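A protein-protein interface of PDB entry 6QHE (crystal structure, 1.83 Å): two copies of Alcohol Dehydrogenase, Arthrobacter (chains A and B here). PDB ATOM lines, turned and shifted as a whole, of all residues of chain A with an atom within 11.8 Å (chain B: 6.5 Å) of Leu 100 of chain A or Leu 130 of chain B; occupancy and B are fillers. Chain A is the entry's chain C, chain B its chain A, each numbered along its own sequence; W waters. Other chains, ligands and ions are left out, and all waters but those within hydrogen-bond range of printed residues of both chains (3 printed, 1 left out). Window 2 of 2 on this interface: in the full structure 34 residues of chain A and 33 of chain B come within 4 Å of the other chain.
The backbone NH of Arg 97 of chain A sits at hydrogen-bond distance from the backbone carbonyl oxygen of Gly 152 of chain A, 2.9 Å away.
The backbone carbonyl oxygen of Phe 174 of chain B sits at hydrogen-bond distance from the backbone NH of Ile 179 of chain B (3.2 Å).
The backbone NH (N) of Phe 99 of chain A lies within hydrogen-bond range of the side-chain carboxylate (OE2) of Glu 173 of chain B.
The backbone NH (N) of Gly 152 of chain A lies within hydrogen-bond range of the side-chain carboxylate (OE1) of Glu 173 of chain B, at 2.8 Å.
The backbone carbonyl oxygen (O) of Leu 100 of chain A is in hydrogen-bond range of the guanidinium group (NH2) of Arg 123 of chain B, 3.1 Å away.
No position is printed for both chains.
Of the 10 pairs that touch across the chains among the printed residues, none has its exchanged pair printed and touching as well.
CE of Met 98 of chain A touches OE2 of Glu 173 of chain B, at 3.4 Å.
Phe 99 of chain A touches Cys 122 of chain B (CZ to CB, 3.95 Å).
CA of Arg 123 of chain B touches CZ of Phe 99 of chain A (3.6 Å).
Phe 99 of chain A touches Phe 174 of chain B (CD2 to CE2, 3.8 Å).
Leu 100 of chain A touches Leu 130 of chain B.
Pro 151 of chain A touches Glu 173 of chain B.
Glu 173 of chain B touches Thr 154 of chain A (OE1 to CG2, 3.8 Å).
Printed residues of chain B within 4 Å of Met 98 of chain A: Glu 173 (3.4 Å).
Of chain B, only Arg 123 (3.1 Å) and Leu 130 (3.9 Å) come within 4 Å of Leu 100 of chain A.
Printed residues of chain B within 4 Å of Pro 151 of chain A: Glu 173.
Printed residues of chain B within 4 Å of Gly 152 of chain A: Glu 173.
Arg 123 of chain B touches just these residues of chain A: Phe 99 and Leu 100.
No residue of chain A comes within 4 Å of Pro 127 of chain B.
No residue of chain A comes within 4 Å of Met 129 of chain B.
Leu 130 of chain B touches just one residue of chain A: Leu 100.
No residue of chain A comes within 4 Å of Asn 132 of chain B.
Lys 133 of chain B touches none of the printed residues of chain A.
Printed residues of chain A within 4 Å of Phe 174 of chain B: Phe 99 (3.8 Å).
No residue of chain A comes within 4 Å of Gln 177 of chain B.
The nearest residue of chain B that does not touch Leu 100 of chain A is Val 126 of chain B (4.1 Å).
The nearest residue of chain A that does not touch Leu 130 of chain B is Phe 99 of chain A (7.8 Å).
The nearest printed residue of chain B that does not touch Phe 99 of chain A is Val 126 of chain B (4.04 Å).
Of the 18 printed residues of chain A, 6 touch a printed residue of chain B.
Hydrophobic or aromatic side chains of chain A that line the printed part of chain B: Met 98, Phe 99, Leu 100 and Pro 151.
Among the printed residues, 10 pairs touch across the chains.
Water W3 lies within hydrogen-bond range of the backbone carbonyl oxygen (O) of Val 102 of chain A (2.7 Å), the backbone carbonyl oxygen (O) of Phe 99 of chain A (2.7 Å) and the guanidinium group (NE) of Arg 123 of chain B (2.8 Å).
Water W1 lies within hydrogen-bond range of OG1 of Thr 154 of chain A (2.7 Å), OE1 of Glu 173 of chain B (2.7 Å), O of Arg 97 of chain A (2.7 Å), N of Phe 99 of chain A (3.1 Å) and N of Trp 153 of chain A (3.3 Å).
Water W2 lies within hydrogen-bond range of OE2 of Glu 173 of chain B, N of Leu 100 of chain A and N of Phe 99 of chain A.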
ATOM      1  N   SER A  96      -1.540 -14.991 -24.915  1.00  0.00           N
ATOM      2  CA  SER A  96      -1.430 -16.429 -24.610  1.00  0.00           C
ATOM      3  C   SER A  96       0.030 -16.855 -24.797  1.00  0.00           C
ATOM      4  O   SER A  96       0.736 -16.313 -25.659  1.00  0.00           O
ATOM      5  CB  SER A  96      -2.338 -17.282 -25.473  1.00  0.00           C
ATOM      6  OG  SER A  96      -1.990 -17.151 -26.803  1.00  0.00           O
ATOM      7  N   ARG A  97       0.483 -17.814 -24.014  1.00  0.00           N
ATOM      8  CA  ARG A  97       1.845 -18.386 -24.090  1.00  0.00           C
ATOM      9  C   ARG A  97       1.833 -19.690 -23.311  1.00  0.00           C
ATOM     10  O   ARG A  97       1.319 -19.692 -22.187  1.00  0.00           O
ATOM     11  CB  ARG A  97       2.842 -17.384 -23.518  1.00  0.00           C
ATOM     12  CG  ARG A  97       4.308 -17.789 -23.624  1.00  0.00           C
ATOM     13  CD  ARG A  97       4.857 -17.524 -25.041  1.00  0.00           C
ATOM     14  NE  ARG A  97       4.890 -16.111 -25.340  1.00  0.00           N
ATOM     15  CZ  ARG A  97       5.817 -15.257 -24.892  1.00  0.00           C
ATOM     16  NH1 ARG A  97       6.789 -15.668 -24.087  1.00  0.00           N
ATOM     17  NH2 ARG A  97       5.734 -13.972 -25.225  1.00  0.00           N
ATOM     18  N   MET A  98       2.379 -20.753 -23.877  1.00  0.00           N
ATOM     19  CA  MET A  98       2.518 -22.040 -23.157  1.00  0.00           C
ATOM     20  C   MET A  98       3.365 -21.781 -21.904  1.00  0.00           C
ATOM     21  O   MET A  98       4.326 -20.957 -21.940  1.00  0.00           O
ATOM     22  CB  MET A  98       3.126 -23.114 -24.054  1.00  0.00           C
ATOM     23  CG  MET A  98       2.244 -23.442 -25.251  1.00  0.00           C
ATOM     24  SD  MET A  98       0.600 -24.150 -24.785  1.00  0.00           S
ATOM     25  CE  MET A  98       1.148 -25.756 -24.218  1.00  0.00           C
ATOM     26  N   PHE A  99       3.008 -22.432 -20.801  1.00  0.00           N
ATOM     27  CA  PHE A  99       3.626 -22.201 -19.476  1.00  0.00           C
ATOM     28  C   PHE A  99       5.172 -22.246 -19.548  1.00  0.00           C
ATOM     29  O   PHE A  99       5.840 -21.350 -19.000  1.00  0.00           O
ATOM     30  CB  PHE A  99       3.114 -23.253 -18.505  1.00  0.00           C
ATOM     31  CG  PHE A  99       3.656 -23.141 -17.110  1.00  0.00           C
ATOM     32  CD1 PHE A  99       3.411 -22.026 -16.331  1.00  0.00           C
ATOM     33  CD2 PHE A  99       4.382 -24.188 -16.580  1.00  0.00           C
ATOM     34  CE1 PHE A  99       3.875 -21.993 -15.020  1.00  0.00           C
ATOM     35  CE2 PHE A  99       4.840 -24.155 -15.276  1.00  0.00           C
ATOM     36  CZ  PHE A  99       4.619 -23.037 -14.515  1.00  0.00           C
ATOM     37  N   LEU A 100       5.725 -23.287 -20.158  1.00  0.00           N
ATOM     38  CA  LEU A 100       7.199 -23.459 -20.191  1.00  0.00           C
ATOM     39  C   LEU A 100       7.851 -22.419 -21.126  1.00  0.00           C
ATOM     40  O   LEU A 100       9.057 -22.215 -20.994  1.00  0.00           O
ATOM     41  CB  LEU A 100       7.528 -24.884 -20.619  1.00  0.00           C
ATOM     42  CG  LEU A 100       7.068 -25.976 -19.646  1.00  0.00           C
ATOM     43  CD1 LEU A 100       7.348 -27.355 -20.209  1.00  0.00           C
ATOM     44  CD2 LEU A 100       7.679 -25.790 -18.266  1.00  0.00           C
ATOM     45  N   ASP A 101       7.098 -21.768 -22.005  1.00  0.00           N
ATOM     46  CA  ASP A 101       7.617 -20.714 -22.917  1.00  0.00           C
ATOM     47  C   ASP A 101       7.437 -19.320 -22.325  1.00  0.00           C
ATOM     48  O   ASP A 101       7.798 -18.356 -22.987  1.00  0.00           O
ATOM     49  CB  ASP A 101       6.917 -20.786 -24.270  1.00  0.00           C
ATOM     50  CG  ASP A 101       7.144 -22.065 -25.026  1.00  0.00           C
ATOM     51  OD1 ASP A 101       8.164 -22.710 -24.792  1.00  0.00           O
ATOM     52  OD2 ASP A 101       6.278 -22.411 -25.835  1.00  0.00           O
ATOM     53  N   VAL A 102       6.796 -19.182 -21.161  1.00  0.00           N
ATOM     54  CA  VAL A 102       6.595 -17.850 -20.556  1.00  0.00           C
ATOM     55  C   VAL A 102       7.959 -17.270 -20.207  1.00  0.00           C
ATOM     56  O   VAL A 102       8.778 -17.973 -19.602  1.00  0.00           O
ATOM     57  CB  VAL A 102       5.681 -17.931 -19.318  1.00  0.00           C
ATOM     58  CG1 VAL A 102       5.742 -16.658 -18.480  1.00  0.00           C
ATOM     59  CG2 VAL A 102       4.256 -18.238 -19.761  1.00  0.00           C
ATOM     60  N   ASP A 103       8.154 -15.993 -20.520  1.00  0.00           N
ATOM     61  CA  ASP A 103       9.338 -15.228 -20.066  1.00  0.00           C
ATOM     62  C   ASP A 103       8.866 -14.098 -19.160  1.00  0.00           C
ATOM     63  O   ASP A 103       7.643 -13.812 -19.137  1.00  0.00           O
ATOM     64  CB  ASP A 103      10.186 -14.750 -21.248  1.00  0.00           C
ATOM     65  CG  ASP A 103       9.405 -13.993 -22.298  1.00  0.00           C
ATOM     66  OD1 ASP A 103       8.460 -13.287 -21.943  1.00  0.00           O
ATOM     67  OD2 ASP A 103       9.719 -14.165 -23.488  1.00  0.00           O
ATOM     68  N   ASP A 104       9.802 -13.456 -18.457  1.00  0.00           N
ATOM     69  CA  ASP A 104       9.482 -12.366 -17.500  1.00  0.00           C
ATOM     70  C   ASP A 104       8.705 -11.261 -18.208  1.00  0.00           C
ATOM     71  O   ASP A 104       7.794 -10.691 -17.576  1.00  0.00           O
ATOM     72  CB  ASP A 104      10.722 -11.861 -16.777  1.00  0.00           C
ATOM     73  CG  ASP A 104      11.252 -12.851 -15.762  1.00  0.00           C
ATOM     74  OD1 ASP A 104      10.589 -13.877 -15.524  1.00  0.00           O
ATOM     75  OD2 ASP A 104      12.329 -12.593 -15.208  1.00  0.00           O
ATOM     76  N   ALA A 105       9.029 -10.936 -19.461  1.00  0.00           N
ATOM     77  CA  ALA A 105       8.359  -9.835 -20.192  1.00  0.00           C
ATOM     78  C   ALA A 105       6.853 -10.134 -20.342  1.00  0.00           C
ATOM     79  O   ALA A 105       6.024  -9.223 -20.141  1.00  0.00           O
ATOM     80  CB  ALA A 105       9.011  -9.617 -21.541  1.00  0.00           C
ATOM     81  N   HIS A 106       6.508 -11.355 -20.728  1.00  0.00           N
ATOM     82  CA  HIS A 106       5.095 -11.772 -20.934  1.00  0.00           C
ATOM     83  C   HIS A 106       4.342 -11.756 -19.593  1.00  0.00           C
ATOM     84  O   HIS A 106       3.236 -11.195 -19.534  1.00  0.00           O
ATOM     85  CB  HIS A 106       5.046 -13.144 -21.577  1.00  0.00           C
ATOM     86  CG  HIS A 106       3.669 -13.719 -21.622  1.00  0.00           C
ATOM     87  ND1 HIS A 106       2.713 -13.273 -22.529  1.00  0.00           N
ATOM     88  CD2 HIS A 106       3.051 -14.609 -20.841  1.00  0.00           C
ATOM     89  CE1 HIS A 106       1.589 -13.957 -22.338  1.00  0.00           C
ATOM     90  NE2 HIS A 106       1.755 -14.775 -21.305  1.00  0.00           N
ATOM     91  N   TYR A 107       4.940 -12.345 -18.572  1.00  0.00           N
ATOM     92  CA  TYR A 107       4.362 -12.424 -17.214  1.00  0.00           C
ATOM     93  C   TYR A 107       4.052 -11.010 -16.755  1.00  0.00           C
ATOM     94  O   TYR A 107       2.942 -10.701 -16.309  1.00  0.00           O
ATOM     95  CB  TYR A 107       5.341 -13.132 -16.276  1.00  0.00           C
ATOM     96  CG  TYR A 107       4.867 -13.308 -14.861  1.00  0.00           C
ATOM     97  CD1 TYR A 107       5.025 -12.309 -13.911  1.00  0.00           C
ATOM     98  CD2 TYR A 107       4.261 -14.488 -14.469  1.00  0.00           C
ATOM     99  CE1 TYR A 107       4.614 -12.496 -12.597  1.00  0.00           C
ATOM    100  CE2 TYR A 107       3.833 -14.688 -13.165  1.00  0.00           C
ATOM    101  CZ  TYR A 107       3.990 -13.685 -12.228  1.00  0.00           C
ATOM    102  OH  TYR A 107       3.558 -13.889 -10.951  1.00  0.00           O
ATOM    103  N   ASP A 150      -8.169 -23.248 -20.971  1.00  0.00           N
ATOM    104  CA  ASP A 150      -7.510 -24.042 -22.031  1.00  0.00           C
ATOM    105  C   ASP A 150      -6.016 -23.978 -21.807  1.00  0.00           C
ATOM    106  O   ASP A 150      -5.492 -23.064 -21.151  1.00  0.00           O
ATOM    107  CB  ASP A 150      -7.857 -23.507 -23.425  1.00  0.00           C
ATOM    108  CG  ASP A 150      -9.041 -24.155 -24.090  1.00  0.00           C
ATOM    109  OD1 ASP A 150      -9.652 -25.086 -23.499  1.00  0.00           O
ATOM    110  OD2 ASP A 150      -9.341 -23.704 -25.219  1.00  0.00           O
ATOM    111  N   PRO A 151      -5.262 -24.917 -22.415  1.00  0.00           N
ATOM    112  CA  PRO A 151      -3.806 -24.829 -22.434  1.00  0.00           C
ATOM    113  C   PRO A 151      -3.354 -23.490 -23.045  1.00  0.00           C
ATOM    114  O   PRO A 151      -3.970 -23.029 -23.979  1.00  0.00           O
ATOM    115  CB  PRO A 151      -3.404 -26.028 -23.327  1.00  0.00           C
ATOM    116  CG  PRO A 151      -4.539 -26.989 -23.132  1.00  0.00           C
ATOM    117  CD  PRO A 151      -5.763 -26.114 -23.121  1.00  0.00           C
ATOM    118  N   GLY A 152      -2.280 -22.901 -22.509  1.00  0.00           N
ATOM    119  CA  GLY A 152      -1.644 -21.725 -23.133  1.00  0.00           C
ATOM    120  C   GLY A 152      -2.136 -20.403 -22.560  1.00  0.00           C
ATOM    121  O   GLY A 152      -1.833 -19.356 -23.114  1.00  0.00           O
ATOM    122  N   TRP A 153      -2.805 -20.437 -21.408  1.00  0.00           N
ATOM    123  CA  TRP A 153      -3.430 -19.239 -20.821  1.00  0.00           C
ATOM    124  C   TRP A 153      -3.068 -19.102 -19.338  1.00  0.00           C
ATOM    125  O   TRP A 153      -3.828 -18.414 -18.642  1.00  0.00           O
ATOM    126  CB  TRP A 153      -4.944 -19.334 -20.979  1.00  0.00           C
ATOM    127  CG  TRP A 153      -5.375 -19.292 -22.407  1.00  0.00           C
ATOM    128  CD1 TRP A 153      -5.674 -20.355 -23.189  1.00  0.00           C
ATOM    129  CD2 TRP A 153      -5.518 -18.128 -23.232  1.00  0.00           C
ATOM    130  NE1 TRP A 153      -6.033 -19.931 -24.432  1.00  0.00           N
ATOM    131  CE2 TRP A 153      -5.909 -18.574 -24.509  1.00  0.00           C
ATOM    132  CE3 TRP A 153      -5.327 -16.756 -23.037  1.00  0.00           C
ATOM    133  CZ2 TRP A 153      -6.102 -17.702 -25.583  1.00  0.00           C
ATOM    134  CZ3 TRP A 153      -5.522 -15.889 -24.094  1.00  0.00           C
ATOM    135  CH2 TRP A 153      -5.913 -16.360 -25.349  1.00  0.00           C
ATOM    136  N   THR A 154      -1.950 -19.642 -18.875  1.00  0.00           N
ATOM    137  CA  THR A 154      -1.624 -19.606 -17.429  1.00  0.00           C
ATOM    138  C   THR A 154      -1.542 -18.174 -16.923  1.00  0.00           C
ATOM    139  O   THR A 154      -2.104 -17.888 -15.829  1.00  0.00           O
ATOM    140  CB  THR A 154      -0.371 -20.409 -17.051  1.00  0.00           C
ATOM    141  OG1 THR A 154       0.726 -20.037 -17.874  1.00  0.00           O
ATOM    142  CG2 THR A 154      -0.607 -21.896 -17.143  1.00  0.00           C
ATOM    143  N   VAL A 155      -0.846 -17.265 -17.622  1.00  0.00           N
ATOM    144  CA  VAL A 155      -0.692 -15.897 -17.058  1.00  0.00           C
ATOM    145  C   VAL A 155      -2.018 -15.151 -17.129  1.00  0.00           C
ATOM    146  O   VAL A 155      -2.386 -14.457 -16.161  1.00  0.00           O
ATOM    147  CB  VAL A 155       0.446 -15.107 -17.722  1.00  0.00           C
ATOM    148  CG1 VAL A 155       0.541 -13.726 -17.120  1.00  0.00           C
ATOM    149  CG2 VAL A 155       1.772 -15.858 -17.562  1.00  0.00           C
ATOM    150  N   LEU B  84      10.943 -36.641  -9.557  1.00  0.00           N
ATOM    151  CA  LEU B  84      10.152 -35.685  -8.734  1.00  0.00           C
ATOM    152  C   LEU B  84       8.675 -35.965  -9.028  1.00  0.00           C
ATOM    153  O   LEU B  84       8.284 -35.879 -10.213  1.00  0.00           O
ATOM    154  CB  LEU B  84      10.527 -34.253  -9.081  1.00  0.00           C
ATOM    155  CG  LEU B  84       9.679 -33.200  -8.365  1.00  0.00           C
ATOM    156  CD1 LEU B  84       9.838 -33.338  -6.871  1.00  0.00           C
ATOM    157  CD2 LEU B  84      10.011 -31.786  -8.790  1.00  0.00           C
ATOM    158  N   CYS B 122       6.245 -24.084  -9.350  1.00  0.00           N
ATOM    159  CA  CYS B 122       5.630 -24.922 -10.404  1.00  0.00           C
ATOM    160  C   CYS B 122       6.557 -24.972 -11.634  1.00  0.00           C
ATOM    161  O   CYS B 122       6.716 -26.067 -12.245  1.00  0.00           O
ATOM    162  CB  CYS B 122       4.260 -24.392 -10.817  1.00  0.00           C
ATOM    163  SG  CYS B 122       3.050 -24.615  -9.488  1.00  0.00           S
ATOM    164  N   ARG B 123       7.122 -23.831 -12.016  1.00  0.00           N
ATOM    165  CA  ARG B 123       7.921 -23.730 -13.263  1.00  0.00           C
ATOM    166  C   ARG B 123       9.202 -24.573 -13.125  1.00  0.00           C
ATOM    167  O   ARG B 123       9.625 -25.158 -14.133  1.00  0.00           O
ATOM    168  CB  ARG B 123       8.171 -22.261 -13.607  1.00  0.00           C
ATOM    169  CG  ARG B 123       9.056 -22.059 -14.833  1.00  0.00           C
ATOM    170  CD  ARG B 123       8.451 -22.746 -16.033  1.00  0.00           C
ATOM    171  NE  ARG B 123       9.281 -22.612 -17.229  1.00  0.00           N
ATOM    172  CZ  ARG B 123      10.301 -23.411 -17.547  1.00  0.00           C
ATOM    173  NH1 ARG B 123      10.668 -24.416 -16.768  1.00  0.00           N
ATOM    174  NH2 ARG B 123      10.908 -23.235 -18.703  1.00  0.00           N
ATOM    175  N   ALA B 125       9.452 -27.303 -11.103  1.00  0.00           N
ATOM    176  CA  ALA B 125       9.050 -28.708 -10.852  1.00  0.00           C
ATOM    177  C   ALA B 125       8.535 -29.396 -12.121  1.00  0.00           C
ATOM    178  O   ALA B 125       8.820 -30.594 -12.308  1.00  0.00           O
ATOM    179  CB  ALA B 125       8.016 -28.776  -9.752  1.00  0.00           C
ATOM    180  N   VAL B 126       7.718 -28.708 -12.916  1.00  0.00           N
ATOM    181  CA  VAL B 126       6.961 -29.344 -14.028  1.00  0.00           C
ATOM    182  C   VAL B 126       7.921 -30.086 -14.967  1.00  0.00           C
ATOM    183  O   VAL B 126       7.624 -31.216 -15.338  1.00  0.00           O
ATOM    184  CB  VAL B 126       6.092 -28.316 -14.770  1.00  0.00           C
ATOM    185  CG1 VAL B 126       5.690 -28.758 -16.168  1.00  0.00           C
ATOM    186  CG2 VAL B 126       4.847 -27.981 -13.967  1.00  0.00           C
ATOM    187  N   PRO B 127       9.089 -29.519 -15.393  1.00  0.00           N
ATOM    188  CA  PRO B 127      10.004 -30.253 -16.284  1.00  0.00           C
ATOM    189  C   PRO B 127      10.387 -31.634 -15.737  1.00  0.00           C
ATOM    190  O   PRO B 127      10.412 -32.593 -16.482  1.00  0.00           O
ATOM    191  CB  PRO B 127      11.240 -29.321 -16.369  1.00  0.00           C
ATOM    192  CG  PRO B 127      10.614 -27.957 -16.238  1.00  0.00           C
ATOM    193  CD  PRO B 127       9.568 -28.158 -15.141  1.00  0.00           C
ATOM    194  N   HIS B 128      10.669 -31.729 -14.444  1.00  0.00           N
ATOM    195  CA  HIS B 128      11.055 -33.001 -13.778  1.00  0.00           C
ATOM    196  C   HIS B 128       9.859 -33.954 -13.716  1.00  0.00           C
ATOM    197  O   HIS B 128      10.035 -35.174 -13.883  1.00  0.00           O
ATOM    198  CB  HIS B 128      11.662 -32.705 -12.423  1.00  0.00           C
ATOM    199  CG  HIS B 128      12.909 -31.909 -12.523  1.00  0.00           C
ATOM    200  ND1 HIS B 128      14.025 -32.393 -13.211  1.00  0.00           N
ATOM    201  CD2 HIS B 128      13.217 -30.665 -12.092  1.00  0.00           C
ATOM    202  CE1 HIS B 128      14.968 -31.471 -13.166  1.00  0.00           C
ATOM    203  NE2 HIS B 128      14.500 -30.406 -12.487  1.00  0.00           N
ATOM    204  N   MET B 129       8.653 -33.434 -13.526  1.00  0.00           N
ATOM    205  CA  MET B 129       7.446 -34.300 -13.559  1.00  0.00           C
ATOM    206  C   MET B 129       7.187 -34.817 -14.977  1.00  0.00           C
ATOM    207  O   MET B 129       6.741 -35.967 -15.113  1.00  0.00           O
ATOM    208  CB  MET B 129       6.229 -33.526 -13.039  1.00  0.00           C
ATOM    209  CG  MET B 129       6.387 -33.172 -11.583  1.00  0.00           C
ATOM    210  SD  MET B 129       5.045 -32.106 -11.029  1.00  0.00           S
ATOM    211  CE  MET B 129       5.368 -32.143  -9.266  1.00  0.00           C
ATOM    212  N   LEU B 130       7.470 -34.025 -15.998  1.00  0.00           N
ATOM    213  CA  LEU B 130       7.319 -34.489 -17.406  1.00  0.00           C
ATOM    214  C   LEU B 130       8.308 -35.629 -17.698  1.00  0.00           C
ATOM    215  O   LEU B 130       7.912 -36.582 -18.362  1.00  0.00           O
ATOM    216  CB  LEU B 130       7.511 -33.306 -18.356  1.00  0.00           C
ATOM    217  CG  LEU B 130       6.413 -32.243 -18.316  1.00  0.00           C
ATOM    218  CD1 LEU B 130       6.739 -31.112 -19.263  1.00  0.00           C
ATOM    219  CD2 LEU B 130       5.092 -32.875 -18.665  1.00  0.00           C
ATOM    220  N   SER B 131       9.548 -35.560 -17.203  1.00  0.00           N
ATOM    221  CA  SER B 131      10.550 -36.653 -17.355  1.00  0.00           C
ATOM    222  C   SER B 131       9.993 -37.944 -16.736  1.00  0.00           C
ATOM    223  O   SER B 131      10.162 -38.996 -17.309  1.00  0.00           O
ATOM    224  CB  SER B 131      11.881 -36.258 -16.758  1.00  0.00           C
ATOM    225  OG  SER B 131      12.470 -37.316 -16.018  1.00  0.00           O
ATOM    226  N   ASN B 132       9.309 -37.814 -15.611  1.00  0.00           N
ATOM    227  CA  ASN B 132       8.708 -38.884 -14.794  1.00  0.00           C
ATOM    228  C   ASN B 132       7.409 -39.410 -15.444  1.00  0.00           C
ATOM    229  O   ASN B 132       6.885 -40.391 -14.913  1.00  0.00           O
ATOM    230  CB  ASN B 132       8.488 -38.204 -13.421  1.00  0.00           C
ATOM    231  CG  ASN B 132       8.237 -39.110 -12.249  1.00  0.00           C
ATOM    232  OD1 ASN B 132       9.023 -40.029 -12.019  1.00  0.00           O
ATOM    233  ND2 ASN B 132       7.233 -38.759 -11.453  1.00  0.00           N
ATOM    234  N   LYS B 133       6.826 -38.693 -16.423  1.00  0.00           N
ATOM    235  CA  LYS B 133       5.469 -38.937 -16.996  1.00  0.00           C
ATOM    236  C   LYS B 133       4.355 -38.909 -15.919  1.00  0.00           C
ATOM    237  O   LYS B 133       3.320 -39.527 -16.123  1.00  0.00           O
ATOM    238  CB  LYS B 133       5.439 -40.284 -17.728  1.00  0.00           C
ATOM    239  CG  LYS B 133       6.473 -40.393 -18.840  1.00  0.00           C
ATOM    240  CD  LYS B 133       5.867 -40.939 -20.140  1.00  0.00           C
ATOM    241  N   HIS B 134       4.553 -38.198 -14.818  1.00  0.00           N
ATOM    242  CA  HIS B 134       3.639 -38.273 -13.637  1.00  0.00           C
ATOM    243  C   HIS B 134       3.957 -37.083 -12.740  1.00  0.00           C
ATOM    244  O   HIS B 134       5.118 -36.926 -12.353  1.00  0.00           O
ATOM    245  CB  HIS B 134       3.843 -39.595 -12.842  1.00  0.00           C
ATOM    246  CG  HIS B 134       3.162 -39.641 -11.518  1.00  0.00           C
ATOM    247  ND1 HIS B 134       1.928 -40.269 -11.367  1.00  0.00           N
ATOM    248  CD2 HIS B 134       3.459 -39.080 -10.299  1.00  0.00           C
ATOM    249  CE1 HIS B 134       1.516 -40.129 -10.109  1.00  0.00           C
ATOM    250  NE2 HIS B 134       2.425 -39.364  -9.439  1.00  0.00           N
ATOM    251  N   GLY B 135       2.951 -36.317 -12.330  1.00  0.00           N
ATOM    252  CA  GLY B 135       3.188 -35.314 -11.297  1.00  0.00           C
ATOM    253  C   GLY B 135       1.912 -34.955 -10.591  1.00  0.00           C
ATOM    254  O   GLY B 135       0.864 -35.078 -11.197  1.00  0.00           O
ATOM    255  N   GLU B 173      -3.581 -27.268 -18.811  1.00  0.00           N
ATOM    256  CA  GLU B 173      -2.426 -27.325 -19.734  1.00  0.00           C
ATOM    257  C   GLU B 173      -1.730 -28.682 -19.612  1.00  0.00           C
ATOM    258  O   GLU B 173      -1.287 -29.206 -20.652  1.00  0.00           O
ATOM    259  CB  GLU B 173      -1.454 -26.180 -19.449  1.00  0.00           C
ATOM    260  CG  GLU B 173      -0.320 -26.119 -20.463  1.00  0.00           C
ATOM    261  CD  GLU B 173       0.262 -24.735 -20.668  1.00  0.00           C
ATOM    262  OE1 GLU B 173      -0.478 -23.733 -20.521  1.00  0.00           O
ATOM    263  OE2 GLU B 173       1.462 -24.651 -20.970  1.00  0.00           O
ATOM    264  N   PHE B 174      -1.612 -29.264 -18.414  1.00  0.00           N
ATOM    265  CA  PHE B 174      -0.789 -30.492 -18.222  1.00  0.00           C
ATOM    266  C   PHE B 174      -1.620 -31.748 -17.952  1.00  0.00           C
ATOM    267  O   PHE B 174      -0.988 -32.801 -17.770  1.00  0.00           O
ATOM    268  CB  PHE B 174       0.285 -30.218 -17.166  1.00  0.00           C
ATOM    269  CG  PHE B 174       1.323 -29.251 -17.678  1.00  0.00           C
ATOM    270  CD1 PHE B 174       2.240 -29.663 -18.630  1.00  0.00           C
ATOM    271  CD2 PHE B 174       1.347 -27.940 -17.258  1.00  0.00           C
ATOM    272  CE1 PHE B 174       3.169 -28.774 -19.161  1.00  0.00           C
ATOM    273  CE2 PHE B 174       2.254 -27.036 -17.791  1.00  0.00           C
ATOM    274  CZ  PHE B 174       3.161 -27.452 -18.767  1.00  0.00           C
ATOM    275  N   GLN B 177      -0.474 -34.687 -19.975  1.00  0.00           N
ATOM    276  CA  GLN B 177       0.859 -35.192 -19.574  1.00  0.00           C
ATOM    277  C   GLN B 177       0.823 -35.771 -18.160  1.00  0.00           C
ATOM    278  O   GLN B 177       1.862 -36.053 -17.607  1.00  0.00           O
ATOM    279  CB  GLN B 177       1.881 -34.075 -19.798  1.00  0.00           C
ATOM    280  CG  GLN B 177       2.051 -33.788 -21.293  1.00  0.00           C
ATOM    281  CD  GLN B 177       2.557 -32.402 -21.611  1.00  0.00           C
ATOM    282  OE1 GLN B 177       1.807 -31.415 -21.662  1.00  0.00           O
ATOM    283  NE2 GLN B 177       3.847 -32.325 -21.882  1.00  0.00           N
ATOM    284  N   ASN B 178      -0.373 -36.002 -17.621  1.00  0.00           N
ATOM    285  CA  ASN B 178      -0.597 -36.724 -16.345  1.00  0.00           C
ATOM    286  C   ASN B 178       0.026 -35.926 -15.196  1.00  0.00           C
ATOM    287  O   ASN B 178       0.565 -36.540 -14.237  1.00  0.00           O
ATOM    288  CB  ASN B 178      -0.089 -38.167 -16.419  1.00  0.00           C
ATOM    289  CG  ASN B 178      -0.550 -38.982 -15.222  1.00  0.00           C
ATOM    290  OD1 ASN B 178      -1.690 -38.784 -14.761  1.00  0.00           O
ATOM    291  ND2 ASN B 178       0.351 -39.816 -14.678  1.00  0.00           N
ATOM    292  N   ILE B 179      -0.006 -34.608 -15.287  1.00  0.00           N
ATOM    293  CA  ILE B 179       0.281 -33.753 -14.098  1.00  0.00           C
ATOM    294  C   ILE B 179      -1.076 -33.209 -13.635  1.00  0.00           C
ATOM    295  O   ILE B 179      -1.714 -32.479 -14.382  1.00  0.00           O
ATOM    296  CB  ILE B 179       1.290 -32.648 -14.394  1.00  0.00           C
ATOM    297  CG1 ILE B 179       2.598 -33.239 -14.944  1.00  0.00           C
ATOM    298  CG2 ILE B 179       1.531 -31.816 -13.147  1.00  0.00           C
ATOM    299  CD1 ILE B 179       3.644 -32.214 -15.303  1.00  0.00           C
HETATM  300  O   HOH W   1       0.186 -21.157 -20.242  1.00  0.00           O
HETATM  301  O   HOH W   2       4.128 -25.420 -21.380  1.00  0.00           O
HETATM  302  O   HOH W   3       8.195 -20.181 -18.240  1.00  0.00           O
